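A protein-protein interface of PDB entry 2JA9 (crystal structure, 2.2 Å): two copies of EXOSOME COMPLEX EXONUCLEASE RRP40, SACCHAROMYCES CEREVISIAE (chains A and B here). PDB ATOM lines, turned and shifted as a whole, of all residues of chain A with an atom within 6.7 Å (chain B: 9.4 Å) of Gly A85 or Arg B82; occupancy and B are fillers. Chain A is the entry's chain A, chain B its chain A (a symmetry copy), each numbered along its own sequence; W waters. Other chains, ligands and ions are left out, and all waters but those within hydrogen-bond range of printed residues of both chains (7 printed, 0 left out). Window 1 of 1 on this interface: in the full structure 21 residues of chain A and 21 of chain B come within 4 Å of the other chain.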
ATOM      1  N   TYR A  59      13.136  -8.470   4.197  1.00  0.00           N
ATOM      2  CA  TYR A  59      14.578  -8.323   4.162  1.00  0.00           C
ATOM      3  C   TYR A  59      15.053  -9.028   2.898  1.00  0.00           C
ATOM      4  O   TYR A  59      14.629 -10.150   2.606  1.00  0.00           O
ATOM      5  CB  TYR A  59      15.221  -8.941   5.408  1.00  0.00           C
ATOM      6  CG  TYR A  59      16.650  -8.499   5.693  1.00  0.00           C
ATOM      7  CD1 TYR A  59      17.015  -7.155   5.641  1.00  0.00           C
ATOM      8  CD2 TYR A  59      17.626  -9.418   6.065  1.00  0.00           C
ATOM      9  CE1 TYR A  59      18.319  -6.746   5.917  1.00  0.00           C
ATOM     10  CE2 TYR A  59      18.937  -9.014   6.344  1.00  0.00           C
ATOM     11  CZ  TYR A  59      19.268  -7.670   6.270  1.00  0.00           C
ATOM     12  OH  TYR A  59      20.557  -7.252   6.549  1.00  0.00           O
ATOM     13  N   ALA A  60      15.922  -8.366   2.145  1.00  0.00           N
ATOM     14  CA  ALA A  60      16.326  -8.868   0.841  1.00  0.00           C
ATOM     15  C   ALA A  60      17.731  -8.413   0.443  1.00  0.00           C
ATOM     16  O   ALA A  60      18.360  -7.593   1.115  1.00  0.00           O
ATOM     17  CB  ALA A  60      15.315  -8.442  -0.215  1.00  0.00           C
ATOM     18  N   CYS A  75      15.314 -12.983  -2.020  1.00  0.00           N
ATOM     19  CA  CYS A  75      15.146 -13.402  -0.632  1.00  0.00           C
ATOM     20  C   CYS A  75      15.639 -14.833  -0.389  1.00  0.00           C
ATOM     21  O   CYS A  75      14.941 -15.663   0.195  1.00  0.00           O
ATOM     22  CB  CYS A  75      13.688 -13.228  -0.212  1.00  0.00           C
ATOM     23  SG  CYS A  75      13.167 -11.496  -0.213  1.00  0.00           S
ATOM     24  N   ARG A  82      19.144 -21.197   0.811  1.00  0.00           N
ATOM     25  CA  ARG A  82      18.255 -21.089   1.968  1.00  0.00           C
ATOM     26  C   ARG A  82      17.881 -19.637   2.226  1.00  0.00           C
ATOM     27  O   ARG A  82      18.498 -18.730   1.673  1.00  0.00           O
ATOM     28  CB  ARG A  82      18.943 -21.679   3.191  1.00  0.00           C
ATOM     29  CG  ARG A  82      19.558 -23.037   2.923  1.00  0.00           C
ATOM     30  CD  ARG A  82      19.913 -23.725   4.202  1.00  0.00           C
ATOM     31  NE  ARG A  82      18.709 -24.134   4.911  1.00  0.00           N
ATOM     32  CZ  ARG A  82      18.623 -24.324   6.227  1.00  0.00           C
ATOM     33  NH1 ARG A  82      19.675 -24.153   7.024  1.00  0.00           N
ATOM     34  NH2 ARG A  82      17.460 -24.695   6.747  1.00  0.00           N
ATOM     35  N   ASP A  83      16.879 -19.409   3.073  1.00  0.00           N
ATOM     36  CA  ASP A  83      16.386 -18.041   3.293  1.00  0.00           C
ATOM     37  C   ASP A  83      17.450 -17.128   3.892  1.00  0.00           C
ATOM     38  O   ASP A  83      17.524 -15.954   3.530  1.00  0.00           O
ATOM     39  CB  ASP A  83      15.092 -18.012   4.133  1.00  0.00           C
ATOM     40  CG  ASP A  83      15.282 -18.536   5.547  1.00  0.00           C
ATOM     41  OD1 ASP A  83      15.744 -17.773   6.432  1.00  0.00           O
ATOM     42  OD2 ASP A  83      14.944 -19.714   5.780  1.00  0.00           O
ATOM     43  N   ALA A  84      18.263 -17.673   4.798  1.00  0.00           N
ATOM     44  CA  ALA A  84      19.372 -16.943   5.429  1.00  0.00           C
ATOM     45  C   ALA A  84      18.960 -15.613   6.046  1.00  0.00           C
ATOM     46  O   ALA A  84      19.729 -14.648   6.022  1.00  0.00           O
ATOM     47  CB  ALA A  84      20.487 -16.728   4.427  1.00  0.00           C
ATOM     48  N   GLY A  85      17.751 -15.549   6.594  1.00  0.00           N
ATOM     49  CA  GLY A  85      17.258 -14.313   7.186  1.00  0.00           C
ATOM     50  C   GLY A  85      16.495 -13.414   6.229  1.00  0.00           C
ATOM     51  O   GLY A  85      15.829 -12.481   6.661  1.00  0.00           O
ATOM     52  N   PHE A  86      16.581 -13.677   4.927  1.00  0.00           N
ATOM     53  CA  PHE A  86      15.799 -12.915   3.972  1.00  0.00           C
ATOM     54  C   PHE A  86      14.356 -13.396   4.011  1.00  0.00           C
ATOM     55  O   PHE A  86      14.078 -14.513   4.430  1.00  0.00           O
ATOM     56  CB  PHE A  86      16.365 -13.030   2.558  1.00  0.00           C
ATOM     57  CG  PHE A  86      17.802 -12.587   2.437  1.00  0.00           C
ATOM     58  CD1 PHE A  86      18.172 -11.293   2.775  1.00  0.00           C
ATOM     59  CD2 PHE A  86      18.774 -13.460   1.980  1.00  0.00           C
ATOM     60  CE1 PHE A  86      19.481 -10.875   2.666  1.00  0.00           C
ATOM     61  CE2 PHE A  86      20.095 -13.052   1.861  1.00  0.00           C
ATOM     62  CZ  PHE A  86      20.449 -11.757   2.205  1.00  0.00           C
ATOM     63  N   GLY A  87      13.442 -12.536   3.576  1.00  0.00           N
ATOM     64  CA  GLY A  87      12.017 -12.827   3.618  1.00  0.00           C
ATOM     65  C   GLY A  87      11.277 -11.862   4.526  1.00  0.00           C
ATOM     66  O   GLY A  87      11.770 -10.770   4.830  1.00  0.00           O
ATOM     67  N   ILE A  88      10.093 -12.280   4.964  1.00  0.00           N
ATOM     68  CA  ILE A  88       9.205 -11.432   5.737  1.00  0.00           C
ATOM     69  C   ILE A  88       9.796 -11.087   7.115  1.00  0.00           C
ATOM     70  O   ILE A  88      10.460 -11.907   7.745  1.00  0.00           O
ATOM     71  CB  ILE A  88       7.782 -12.068   5.883  1.00  0.00           C
ATOM     72  CG1 ILE A  88       6.777 -11.023   6.383  1.00  0.00           C
ATOM     73  CG2 ILE A  88       7.810 -13.321   6.794  1.00  0.00           C
ATOM     74  CD1 ILE A  88       5.353 -11.510   6.424  1.00  0.00           C
ATOM     75  N   LEU A  89       9.576  -9.852   7.548  1.00  0.00           N
ATOM     76  CA  LEU A  89       9.958  -9.406   8.880  1.00  0.00           C
ATOM     77  C   LEU A  89       8.677  -9.117   9.642  1.00  0.00           C
ATOM     78  O   LEU A  89       7.948  -8.177   9.317  1.00  0.00           O
ATOM     79  CB  LEU A  89      10.829  -8.157   8.793  1.00  0.00           C
ATOM     80  CG  LEU A  89      12.202  -8.324   8.135  1.00  0.00           C
ATOM     81  CD1 LEU A  89      12.861  -6.983   7.956  1.00  0.00           C
ATOM     82  CD2 LEU A  89      13.100  -9.252   8.942  1.00  0.00           C
ATOM     83  N   GLU A  90       8.398  -9.926  10.659  1.00  0.00           N
ATOM     84  CA  GLU A  90       7.145  -9.818  11.401  1.00  0.00           C
ATOM     85  C   GLU A  90       7.343  -9.445  12.850  1.00  0.00           C
ATOM     86  O   GLU A  90       8.276  -9.914  13.487  1.00  0.00           O
ATOM     87  CB  GLU A  90       6.410 -11.151  11.365  1.00  0.00           C
ATOM     88  CG  GLU A  90       6.015 -11.580   9.997  1.00  0.00           C
ATOM     89  CD  GLU A  90       5.336 -12.926  10.016  1.00  0.00           C
ATOM     90  OE1 GLU A  90       6.032 -13.937  10.294  1.00  0.00           O
ATOM     91  OE2 GLU A  90       4.112 -12.955   9.763  1.00  0.00           O
ATOM     92  N   PHE A 123      17.778  -9.756  21.353  1.00  0.00           N
ATOM     93  CA  PHE A 123      17.030  -9.151  20.266  1.00  0.00           C
ATOM     94  C   PHE A 123      17.349  -9.867  18.969  1.00  0.00           C
ATOM     95  O   PHE A 123      18.337 -10.603  18.877  1.00  0.00           O
ATOM     96  CB  PHE A 123      17.370  -7.659  20.136  1.00  0.00           C
ATOM     97  CG  PHE A 123      18.826  -7.387  19.907  1.00  0.00           C
ATOM     98  CD1 PHE A 123      19.670  -7.131  20.967  1.00  0.00           C
ATOM     99  CD2 PHE A 123      19.359  -7.407  18.627  1.00  0.00           C
ATOM    100  CE1 PHE A 123      21.011  -6.890  20.762  1.00  0.00           C
ATOM    101  CE2 PHE A 123      20.710  -7.174  18.417  1.00  0.00           C
ATOM    102  CZ  PHE A 123      21.532  -6.908  19.491  1.00  0.00           C
ATOM    103  N   GLU A 124      16.481  -9.674  17.991  1.00  0.00           N
ATOM    104  CA  GLU A 124      16.794  -9.965  16.610  1.00  0.00           C
ATOM    105  C   GLU A 124      16.923  -8.644  15.893  1.00  0.00           C
ATOM    106  O   GLU A 124      16.111  -7.738  16.106  1.00  0.00           O
ATOM    107  CB  GLU A 124      15.684 -10.777  15.956  1.00  0.00           C
ATOM    108  CG  GLU A 124      15.532 -12.154  16.531  1.00  0.00           C
ATOM    109  CD  GLU A 124      14.487 -12.981  15.806  1.00  0.00           C
ATOM    110  OE1 GLU A 124      14.333 -12.829  14.575  1.00  0.00           O
ATOM    111  OE2 GLU A 124      13.836 -13.812  16.469  1.00  0.00           O
ATOM    112  N   VAL A 125      17.937  -8.535  15.041  1.00  0.00           N
ATOM    113  CA  VAL A 125      18.139  -7.342  14.237  1.00  0.00           C
ATOM    114  C   VAL A 125      18.388  -7.684  12.755  1.00  0.00           C
ATOM    115  O   VAL A 125      19.070  -8.660  12.429  1.00  0.00           O
ATOM    116  CB  VAL A 125      19.303  -6.484  14.802  1.00  0.00           C
ATOM    117  CG1 VAL A 125      20.658  -7.166  14.581  1.00  0.00           C
ATOM    118  CG2 VAL A 125      19.302  -5.095  14.187  1.00  0.00           C
ATOM    119  N   ALA A 126      17.813  -6.865  11.879  1.00  0.00           N
ATOM    120  CA  ALA A 126      18.113  -6.882  10.456  1.00  0.00           C
ATOM    121  C   ALA A 126      18.464  -5.458  10.032  1.00  0.00           C
ATOM    122  O   ALA A 126      17.768  -4.512  10.396  1.00  0.00           O
ATOM    123  CB  ALA A 126      16.920  -7.406   9.655  1.00  0.00           C
ATOM    124  N   TRP A 134      15.619  -2.940  11.470  1.00  0.00           N
ATOM    125  CA  TRP A 134      14.501  -3.681  12.034  1.00  0.00           C
ATOM    126  C   TRP A 134      14.973  -4.375  13.291  1.00  0.00           C
ATOM    127  O   TRP A 134      16.023  -4.999  13.291  1.00  0.00           O
ATOM    128  CB  TRP A 134      14.009  -4.708  11.039  1.00  0.00           C
ATOM    129  CG  TRP A 134      12.894  -5.560  11.518  1.00  0.00           C
ATOM    130  CD1 TRP A 134      11.570  -5.255  11.491  1.00  0.00           C
ATOM    131  CD2 TRP A 134      12.993  -6.882  12.071  1.00  0.00           C
ATOM    132  NE1 TRP A 134      10.837  -6.297  11.994  1.00  0.00           N
ATOM    133  CE2 TRP A 134      11.683  -7.311  12.356  1.00  0.00           C
ATOM    134  CE3 TRP A 134      14.064  -7.743  12.355  1.00  0.00           C
ATOM    135  CZ2 TRP A 134      11.406  -8.566  12.906  1.00  0.00           C
ATOM    136  CZ3 TRP A 134      13.792  -8.992  12.896  1.00  0.00           C
ATOM    137  CH2 TRP A 134      12.470  -9.391  13.165  1.00  0.00           C
ATOM    138  N   LYS A 136      13.527  -6.700  16.904  1.00  0.00           N
ATOM    139  CA  LYS A 136      12.460  -7.432  17.570  1.00  0.00           C
ATOM    140  C   LYS A 136      12.994  -8.142  18.798  1.00  0.00           C
ATOM    141  O   LYS A 136      14.019  -8.820  18.728  1.00  0.00           O
ATOM    142  CB  LYS A 136      11.837  -8.461  16.626  1.00  0.00           C
ATOM    143  CG  LYS A 136      10.781  -9.325  17.301  1.00  0.00           C
ATOM    144  CD  LYS A 136       9.898 -10.061  16.314  1.00  0.00           C
ATOM    145  CE  LYS A 136      10.500 -11.386  15.876  1.00  0.00           C
ATOM    146  NZ  LYS A 136       9.718 -12.030  14.756  1.00  0.00           N
ATOM    147  N   ALA B  40      19.536 -21.431  23.728  1.00  0.00           N
ATOM    148  CA  ALA B  40      20.440 -21.192  22.590  1.00  0.00           C
ATOM    149  C   ALA B  40      19.690 -21.047  21.259  1.00  0.00           C
ATOM    150  O   ALA B  40      20.084 -21.623  20.240  1.00  0.00           O
ATOM    151  CB  ALA B  40      21.477 -22.305  22.504  1.00  0.00           C
ATOM    152  N   PHE B  41      18.619 -20.258  21.284  1.00  0.00           N
ATOM    153  CA  PHE B  41      17.774 -20.007  20.125  1.00  0.00           C
ATOM    154  C   PHE B  41      17.430 -18.507  20.087  1.00  0.00           C
ATOM    155  O   PHE B  41      17.618 -17.813  21.083  1.00  0.00           O
ATOM    156  CB  PHE B  41      16.507 -20.856  20.226  1.00  0.00           C
ATOM    157  CG  PHE B  41      16.758 -22.336  20.096  1.00  0.00           C
ATOM    158  CD1 PHE B  41      16.683 -22.959  18.861  1.00  0.00           C
ATOM    159  CD2 PHE B  41      17.085 -23.101  21.206  1.00  0.00           C
ATOM    160  CE1 PHE B  41      16.920 -24.315  18.732  1.00  0.00           C
ATOM    161  CE2 PHE B  41      17.325 -24.462  21.086  1.00  0.00           C
ATOM    162  CZ  PHE B  41      17.240 -25.070  19.843  1.00  0.00           C
ATOM    163  N   PRO B  42      16.957 -17.996  18.936  1.00  0.00           N
ATOM    164  CA  PRO B  42      16.610 -16.568  18.821  1.00  0.00           C
ATOM    165  C   PRO B  42      15.601 -16.070  19.863  1.00  0.00           C
ATOM    166  O   PRO B  42      14.535 -16.662  20.008  1.00  0.00           O
ATOM    167  CB  PRO B  42      16.020 -16.470  17.407  1.00  0.00           C
ATOM    168  CG  PRO B  42      16.661 -17.558  16.671  1.00  0.00           C
ATOM    169  CD  PRO B  42      16.751 -18.693  17.656  1.00  0.00           C
ATOM    170  N   ASN B  43      15.946 -14.992  20.571  1.00  0.00           N
ATOM    171  CA  ASN B  43      15.093 -14.419  21.623  1.00  0.00           C
ATOM    172  C   ASN B  43      14.563 -15.453  22.632  1.00  0.00           C
ATOM    173  O   ASN B  43      13.432 -15.340  23.114  1.00  0.00           O
ATOM    174  CB  ASN B  43      13.928 -13.630  20.997  1.00  0.00           C
ATOM    175  CG  ASN B  43      14.379 -12.349  20.317  1.00  0.00           C
ATOM    176  OD1 ASN B  43      15.547 -11.973  20.396  1.00  0.00           O
ATOM    177  ND2 ASN B  43      13.453 -11.668  19.649  1.00  0.00           N
ATOM    178  N   ALA B  44      15.387 -16.445  22.958  1.00  0.00           N
ATOM    179  CA  ALA B  44      14.954 -17.539  23.832  1.00  0.00           C
ATOM    180  C   ALA B  44      14.879 -17.114  25.295  1.00  0.00           C
ATOM    181  O   ALA B  44      15.765 -16.424  25.804  1.00  0.00           O
ATOM    182  CB  ALA B  44      15.875 -18.738  23.683  1.00  0.00           C
ATOM    183  N   ARG B  61      25.881 -24.374  15.625  1.00  0.00           N
ATOM    184  CA  ARG B  61      27.207 -23.803  15.691  1.00  0.00           C
ATOM    185  C   ARG B  61      27.830 -24.243  17.017  1.00  0.00           C
ATOM    186  O   ARG B  61      27.215 -24.092  18.071  1.00  0.00           O
ATOM    187  CB  ARG B  61      27.059 -22.277  15.623  1.00  0.00           C
ATOM    188  CG  ARG B  61      28.272 -21.460  15.953  1.00  0.00           C
ATOM    189  CD  ARG B  61      27.984 -19.960  15.762  1.00  0.00           C
ATOM    190  NE  ARG B  61      26.822 -19.502  16.534  1.00  0.00           N
ATOM    191  CZ  ARG B  61      26.830 -19.209  17.839  1.00  0.00           C
ATOM    192  NH1 ARG B  61      27.942 -19.327  18.568  1.00  0.00           N
ATOM    193  NH2 ARG B  61      25.712 -18.802  18.431  1.00  0.00           N
ATOM    194  N   GLU B  74      24.862 -24.066  19.533  1.00  0.00           N
ATOM    195  CA  GLU B  74      23.820 -23.045  19.549  1.00  0.00           C
ATOM    196  C   GLU B  74      23.143 -22.930  18.193  1.00  0.00           C
ATOM    197  O   GLU B  74      23.749 -23.225  17.162  1.00  0.00           O
ATOM    198  CB  GLU B  74      24.403 -21.696  19.960  1.00  0.00           C
ATOM    199  CG  GLU B  74      24.964 -21.717  21.352  1.00  0.00           C
ATOM    200  CD  GLU B  74      25.320 -20.347  21.880  1.00  0.00           C
ATOM    201  OE1 GLU B  74      26.005 -19.598  21.152  1.00  0.00           O
ATOM    202  OE2 GLU B  74      24.929 -20.036  23.032  1.00  0.00           O
ATOM    203  N   CYS B  75      21.891 -22.483  18.213  1.00  0.00           N
ATOM    204  CA  CYS B  75      21.088 -22.365  17.000  1.00  0.00           C
ATOM    205  C   CYS B  75      20.606 -20.929  16.755  1.00  0.00           C
ATOM    206  O   CYS B  75      19.427 -20.679  16.509  1.00  0.00           O
ATOM    207  CB  CYS B  75      19.921 -23.349  17.052  1.00  0.00           C
ATOM    208  SG  CYS B  75      20.468 -25.074  17.050  1.00  0.00           S
ATOM    209  N   PHE B  76      21.551 -19.992  16.814  1.00  0.00           N
ATOM    210  CA  PHE B  76      21.302 -18.607  16.444  1.00  0.00           C
ATOM    211  C   PHE B  76      22.615 -17.938  16.022  1.00  0.00           C
ATOM    212  O   PHE B  76      23.697 -18.461  16.269  1.00  0.00           O
ATOM    213  CB  PHE B  76      20.630 -17.850  17.594  1.00  0.00           C
ATOM    214  CG  PHE B  76      21.537 -17.580  18.771  1.00  0.00           C
ATOM    215  CD1 PHE B  76      21.771 -18.559  19.725  1.00  0.00           C
ATOM    216  CD2 PHE B  76      22.148 -16.339  18.925  1.00  0.00           C
ATOM    217  CE1 PHE B  76      22.605 -18.315  20.804  1.00  0.00           C
ATOM    218  CE2 PHE B  76      22.985 -16.085  20.003  1.00  0.00           C
ATOM    219  CZ  PHE B  76      23.214 -17.076  20.947  1.00  0.00           C
ATOM    220  N   ASP B  77      22.496 -16.796  15.358  1.00  0.00           N
ATOM    221  CA  ASP B  77      23.639 -15.991  14.938  1.00  0.00           C
ATOM    222  C   ASP B  77      24.030 -15.090  16.090  1.00  0.00           C
ATOM    223  O   ASP B  77      23.186 -14.370  16.611  1.00  0.00           O
ATOM    224  CB  ASP B  77      23.241 -15.143  13.729  1.00  0.00           C
ATOM    225  CG  ASP B  77      24.398 -14.358  13.135  1.00  0.00           C
ATOM    226  OD1 ASP B  77      24.929 -13.430  13.787  1.00  0.00           O
ATOM    227  OD2 ASP B  77      24.751 -14.650  11.981  1.00  0.00           O
ATOM    228  N   SER B  78      25.304 -15.127  16.481  1.00  0.00           N
ATOM    229  CA  SER B  78      25.810 -14.308  17.605  1.00  0.00           C
ATOM    230  C   SER B  78      25.695 -12.809  17.359  1.00  0.00           C
ATOM    231  O   SER B  78      25.517 -12.034  18.302  1.00  0.00           O
ATOM    232  CB  SER B  78      27.276 -14.648  17.914  1.00  0.00           C
ATOM    233  OG  SER B  78      27.446 -16.044  18.117  1.00  0.00           O
ATOM    234  N   THR B  79      25.811 -12.390  16.101  1.00  0.00           N
ATOM    235  CA  THR B  79      25.720 -10.963  15.774  1.00  0.00           C
ATOM    236  C   THR B  79      24.254 -10.522  15.696  1.00  0.00           C
ATOM    237  O   THR B  79      23.837  -9.632  16.433  1.00  0.00           O
ATOM    238  CB  THR B  79      26.420 -10.619  14.431  1.00  0.00           C
ATOM    239  OG1 THR B  79      27.709 -11.240  14.376  1.00  0.00           O
ATOM    240  CG2 THR B  79      26.586  -9.112  14.281  1.00  0.00           C
ATOM    241  N   THR B  80      23.479 -11.159  14.817  1.00  0.00           N
ATOM    242  CA  THR B  80      22.123 -10.694  14.527  1.00  0.00           C
ATOM    243  C   THR B  80      21.073 -11.155  15.544  1.00  0.00           C
ATOM    244  O   THR B  80      20.041 -10.506  15.706  1.00  0.00           O
ATOM    245  CB  THR B  80      21.685 -11.076  13.106  1.00  0.00           C
ATOM    246  OG1 THR B  80      21.635 -12.496  12.969  1.00  0.00           O
ATOM    247  CG2 THR B  80      22.660 -10.515  12.084  1.00  0.00           C
ATOM    248  N   GLY B  81      21.346 -12.256  16.234  1.00  0.00           N
ATOM    249  CA  GLY B  81      20.387 -12.862  17.152  1.00  0.00           C
ATOM    250  C   GLY B  81      19.318 -13.688  16.449  1.00  0.00           C
ATOM    251  O   GLY B  81      18.401 -14.196  17.087  1.00  0.00           O
ATOM    252  N   ARG B  82      19.449 -13.840  15.132  1.00  0.00           N
ATOM    253  CA  ARG B  82      18.451 -14.531  14.315  1.00  0.00           C
ATOM    254  C   ARG B  82      18.875 -15.968  14.048  1.00  0.00           C
ATOM    255  O   ARG B  82      20.024 -16.329  14.283  1.00  0.00           O
ATOM    256  CB  ARG B  82      18.270 -13.785  13.001  1.00  0.00           C
ATOM    257  CG  ARG B  82      18.087 -12.293  13.191  1.00  0.00           C
ATOM    258  CD  ARG B  82      17.576 -11.652  11.940  1.00  0.00           C
ATOM    259  NE  ARG B  82      16.196 -12.043  11.697  1.00  0.00           N
ATOM    260  CZ  ARG B  82      15.604 -12.062  10.503  1.00  0.00           C
ATOM    261  NH1 ARG B  82      16.257 -11.706   9.399  1.00  0.00           N
ATOM    262  NH2 ARG B  82      14.335 -12.442  10.420  1.00  0.00           N
ATOM    263  N   ASP B  83      17.955 -16.789  13.546  1.00  0.00           N
ATOM    264  CA  ASP B  83      18.252 -18.217  13.361  1.00  0.00           C
ATOM    265  C   ASP B  83      19.384 -18.452  12.368  1.00  0.00           C
ATOM    266  O   ASP B  83      20.199 -19.351  12.570  1.00  0.00           O
ATOM    267  CB  ASP B  83      17.000 -19.033  12.980  1.00  0.00           C
ATOM    268  CG  ASP B  83      16.409 -18.633  11.639  1.00  0.00           C
ATOM    269  OD1 ASP B  83      16.902 -19.102  10.581  1.00  0.00           O
ATOM    270  OD2 ASP B  83      15.427 -17.863  11.641  1.00  0.00           O
ATOM    271  N   ALA B  84      19.427 -17.644  11.308  1.00  0.00           N
ATOM    272  CA  ALA B  84      20.482 -17.706  10.288  1.00  0.00           C
ATOM    273  C   ALA B  84      20.694 -19.096   9.706  1.00  0.00           C
ATOM    274  O   ALA B  84      21.826 -19.474   9.387  1.00  0.00           O
ATOM    275  CB  ALA B  84      21.781 -17.173  10.854  1.00  0.00           C
ATOM    276  N   GLY B  85      19.620 -19.866   9.568  1.00  0.00           N
ATOM    277  CA  GLY B  85      19.726 -21.220   9.046  1.00  0.00           C
ATOM    278  C   GLY B  85      19.935 -22.292  10.105  1.00  0.00           C
ATOM    279  O   GLY B  85      19.792 -23.474   9.817  1.00  0.00           O
ATOM    280  N   PHE B  86      20.273 -21.898  11.328  1.00  0.00           N
ATOM    281  CA  PHE B  86      20.389 -22.865  12.405  1.00  0.00           C
ATOM    282  C   PHE B  86      18.998 -23.261  12.874  1.00  0.00           C
ATOM    283  O   PHE B  86      18.038 -22.525  12.679  1.00  0.00           O
ATOM    284  CB  PHE B  86      21.216 -22.319  13.567  1.00  0.00           C
ATOM    285  CG  PHE B  86      22.609 -21.888  13.180  1.00  0.00           C
ATOM    286  CD1 PHE B  86      23.495 -22.795  12.615  1.00  0.00           C
ATOM    287  CD2 PHE B  86      23.028 -20.586  13.386  1.00  0.00           C
ATOM    288  CE1 PHE B  86      24.772 -22.414  12.257  1.00  0.00           C
ATOM    289  CE2 PHE B  86      24.310 -20.190  13.036  1.00  0.00           C
ATOM    290  CZ  PHE B  86      25.184 -21.106  12.471  1.00  0.00           C
ATOM    291  N   GLY B  87      18.902 -24.432  13.493  1.00  0.00           N
ATOM    292  CA  GLY B  87      17.626 -24.975  13.936  1.00  0.00           C
ATOM    293  C   GLY B  87      17.293 -26.271  13.221  1.00  0.00           C
ATOM    294  O   GLY B  87      18.176 -26.938  12.671  1.00  0.00           O
HETATM  295  O   HOH W   1      13.256 -12.644   7.503  1.00  0.00           O
HETATM  296  O   HOH W   2      15.238 -15.755  13.380  1.00  0.00           O
HETATM  297  O   HOH W   3      17.974 -15.673   9.938  1.00  0.00           O
HETATM  298  O   HOH W   4      17.444 -24.832   9.861  1.00  0.00           O
HETATM  299  O   HOH W   5      12.149 -13.183  12.893  1.00  0.00           O
HETATM  300  O   HOH W   6      18.658 -19.970   6.358  1.00  0.00           O
HETATM  301  O   HOH W   7      18.120 -13.483  19.468  1.00  0.00           O
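Water W4 lies within hydrogen-bond range of O of Gly B85 (2.7 Å) and NH2 of Arg A82 (3.1 Å).
Water W1 lies within hydrogen-bond range of O of Gly A85 (2.7 Å), O of Ile A88 (2.9 Å) and NH2 of Arg B82 (3.1 Å).
Water W2 bridges OD2 of Asp B83 (2.7 Å) and OE1 of Glu A124 (3.3 Å).
Water W5 lies within hydrogen-bond range of the side-chain carboxylate of Glu A124 (2.8 Å), the side-chain amino group of Lys A136 (3.3 Å) and the guanidinium group of Arg B82 (3.4 Å).
Water W6 bridges N of Ala A84 (2.8 Å) and N of Gly B85 (3.4 Å).
Water W3 lies within hydrogen-bond range of the backbone NH of Ala B84 and the backbone NH of Gly A85.
NH1 of Arg A82 lies within hydrogen-bond range of O of Gly B85, at 2.9 Å.
The guanidinium group of Arg B82 sits at hydrogen-bond distance from the backbone carbonyl oxygen of Gly A85, at 2.9 Å.
The backbone NH (N) of Phe A123 sits close to the side-chain amide oxygen (OD1) of Asn B43 (3.3 Å).
The backbone NH (N) of Glu A124 lies within hydrogen-bond range of the side-chain amide oxygen (OD1) of Asn B43.
OE1 of Glu A124 lies within salt-bridge range of NE of Arg B82, 3.5 Å away.
The backbone NH (N) of Val A125 lies within hydrogen-bond range of the backbone carbonyl oxygen (O) of Thr B80 (3.0 Å).
O of Lys A136 lies within hydrogen-bond range of ND2 of Asn B43 (3.0 Å).
The side-chain carboxylate (OD1) of Asp A83 is in hydrogen-bond range of the backbone NH (N) of Gly A85, 3.0 Å away.
The backbone carbonyl oxygen (O) of Glu A90 is in hydrogen-bond range of the side-chain amino group (NZ) of Lys A136 (2.9 Å).
N of Thr B80 lies within hydrogen-bond range of OD1 of Asp B77 (2.9 Å).
The backbone NH (N) of Asp B77 lies within hydrogen-bond range of the backbone carbonyl oxygen (O) of Arg B82, 2.7 Å away.
The side-chain hydroxyl (OG1) of Thr B80 sits close to the backbone NH (N) of Arg B82, at 3.4 Å.
OD1 of Asp B83 is in hydrogen-bond range of N of Gly B85 (3.0 Å).
Arg A82 touches Gly B85, and with the chains exchanged Gly A85 touches Arg B82.
7 positions are printed for both chains.
Of the 14 pairs that touch across the chains among the printed residues, 2 have their exchanged pair printed and touching as well.
Among the printed residues, merely in contact across the chains: Val A125 with Arg B82, Glu A124 with Thr B80, Phe A123 with Gly B81, Glu A124 with Gly B81, Glu A124 with Pro B42, Phe A123 with Thr B80 and Leu A89 with Arg B82.
Of the 18 printed residues of chain A, 7 touch a printed residue of chain B.
Hydrophobic or aromatic side chains of chain B that line the printed part of chain A: Pro B42.
Among the printed residues, 14 pairs touch across the chains.
Gly A85 touches just one residue of chain B: Arg B82.
No residue of chain B comes within 4 Å of Gly A87.
Of the printed residues of chain B, Val A125 touches Thr B80 (3.0 Å) and Arg B82 (3.4 Å).
Of the printed residues of chain B, Lys A136 touches Asn B43 (3.0 Å).
Printed residues of chain A within 4 Å of Pro B42: Glu A124 (3.6 Å).
Phe B76 touches none of the printed residues of chain A.
Of the printed residues of chain A, Thr B80 touches Phe A123 (3.6 Å), Glu A124 (3.4 Å) and Val A125 (3.0 Å).
Of the printed residues of chain A, Gly B81 touches Phe A123 and Glu A124.
Of chain A, only Gly A85 (2.9 Å), Leu A89 (3.7 Å), Glu A124 (3.5 Å) and Val A125 (3.4 Å) come within 4 Å of Arg B82.
The nearest residue of chain B that does not touch Gly A85 is Ala B84 (5.1 Å).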
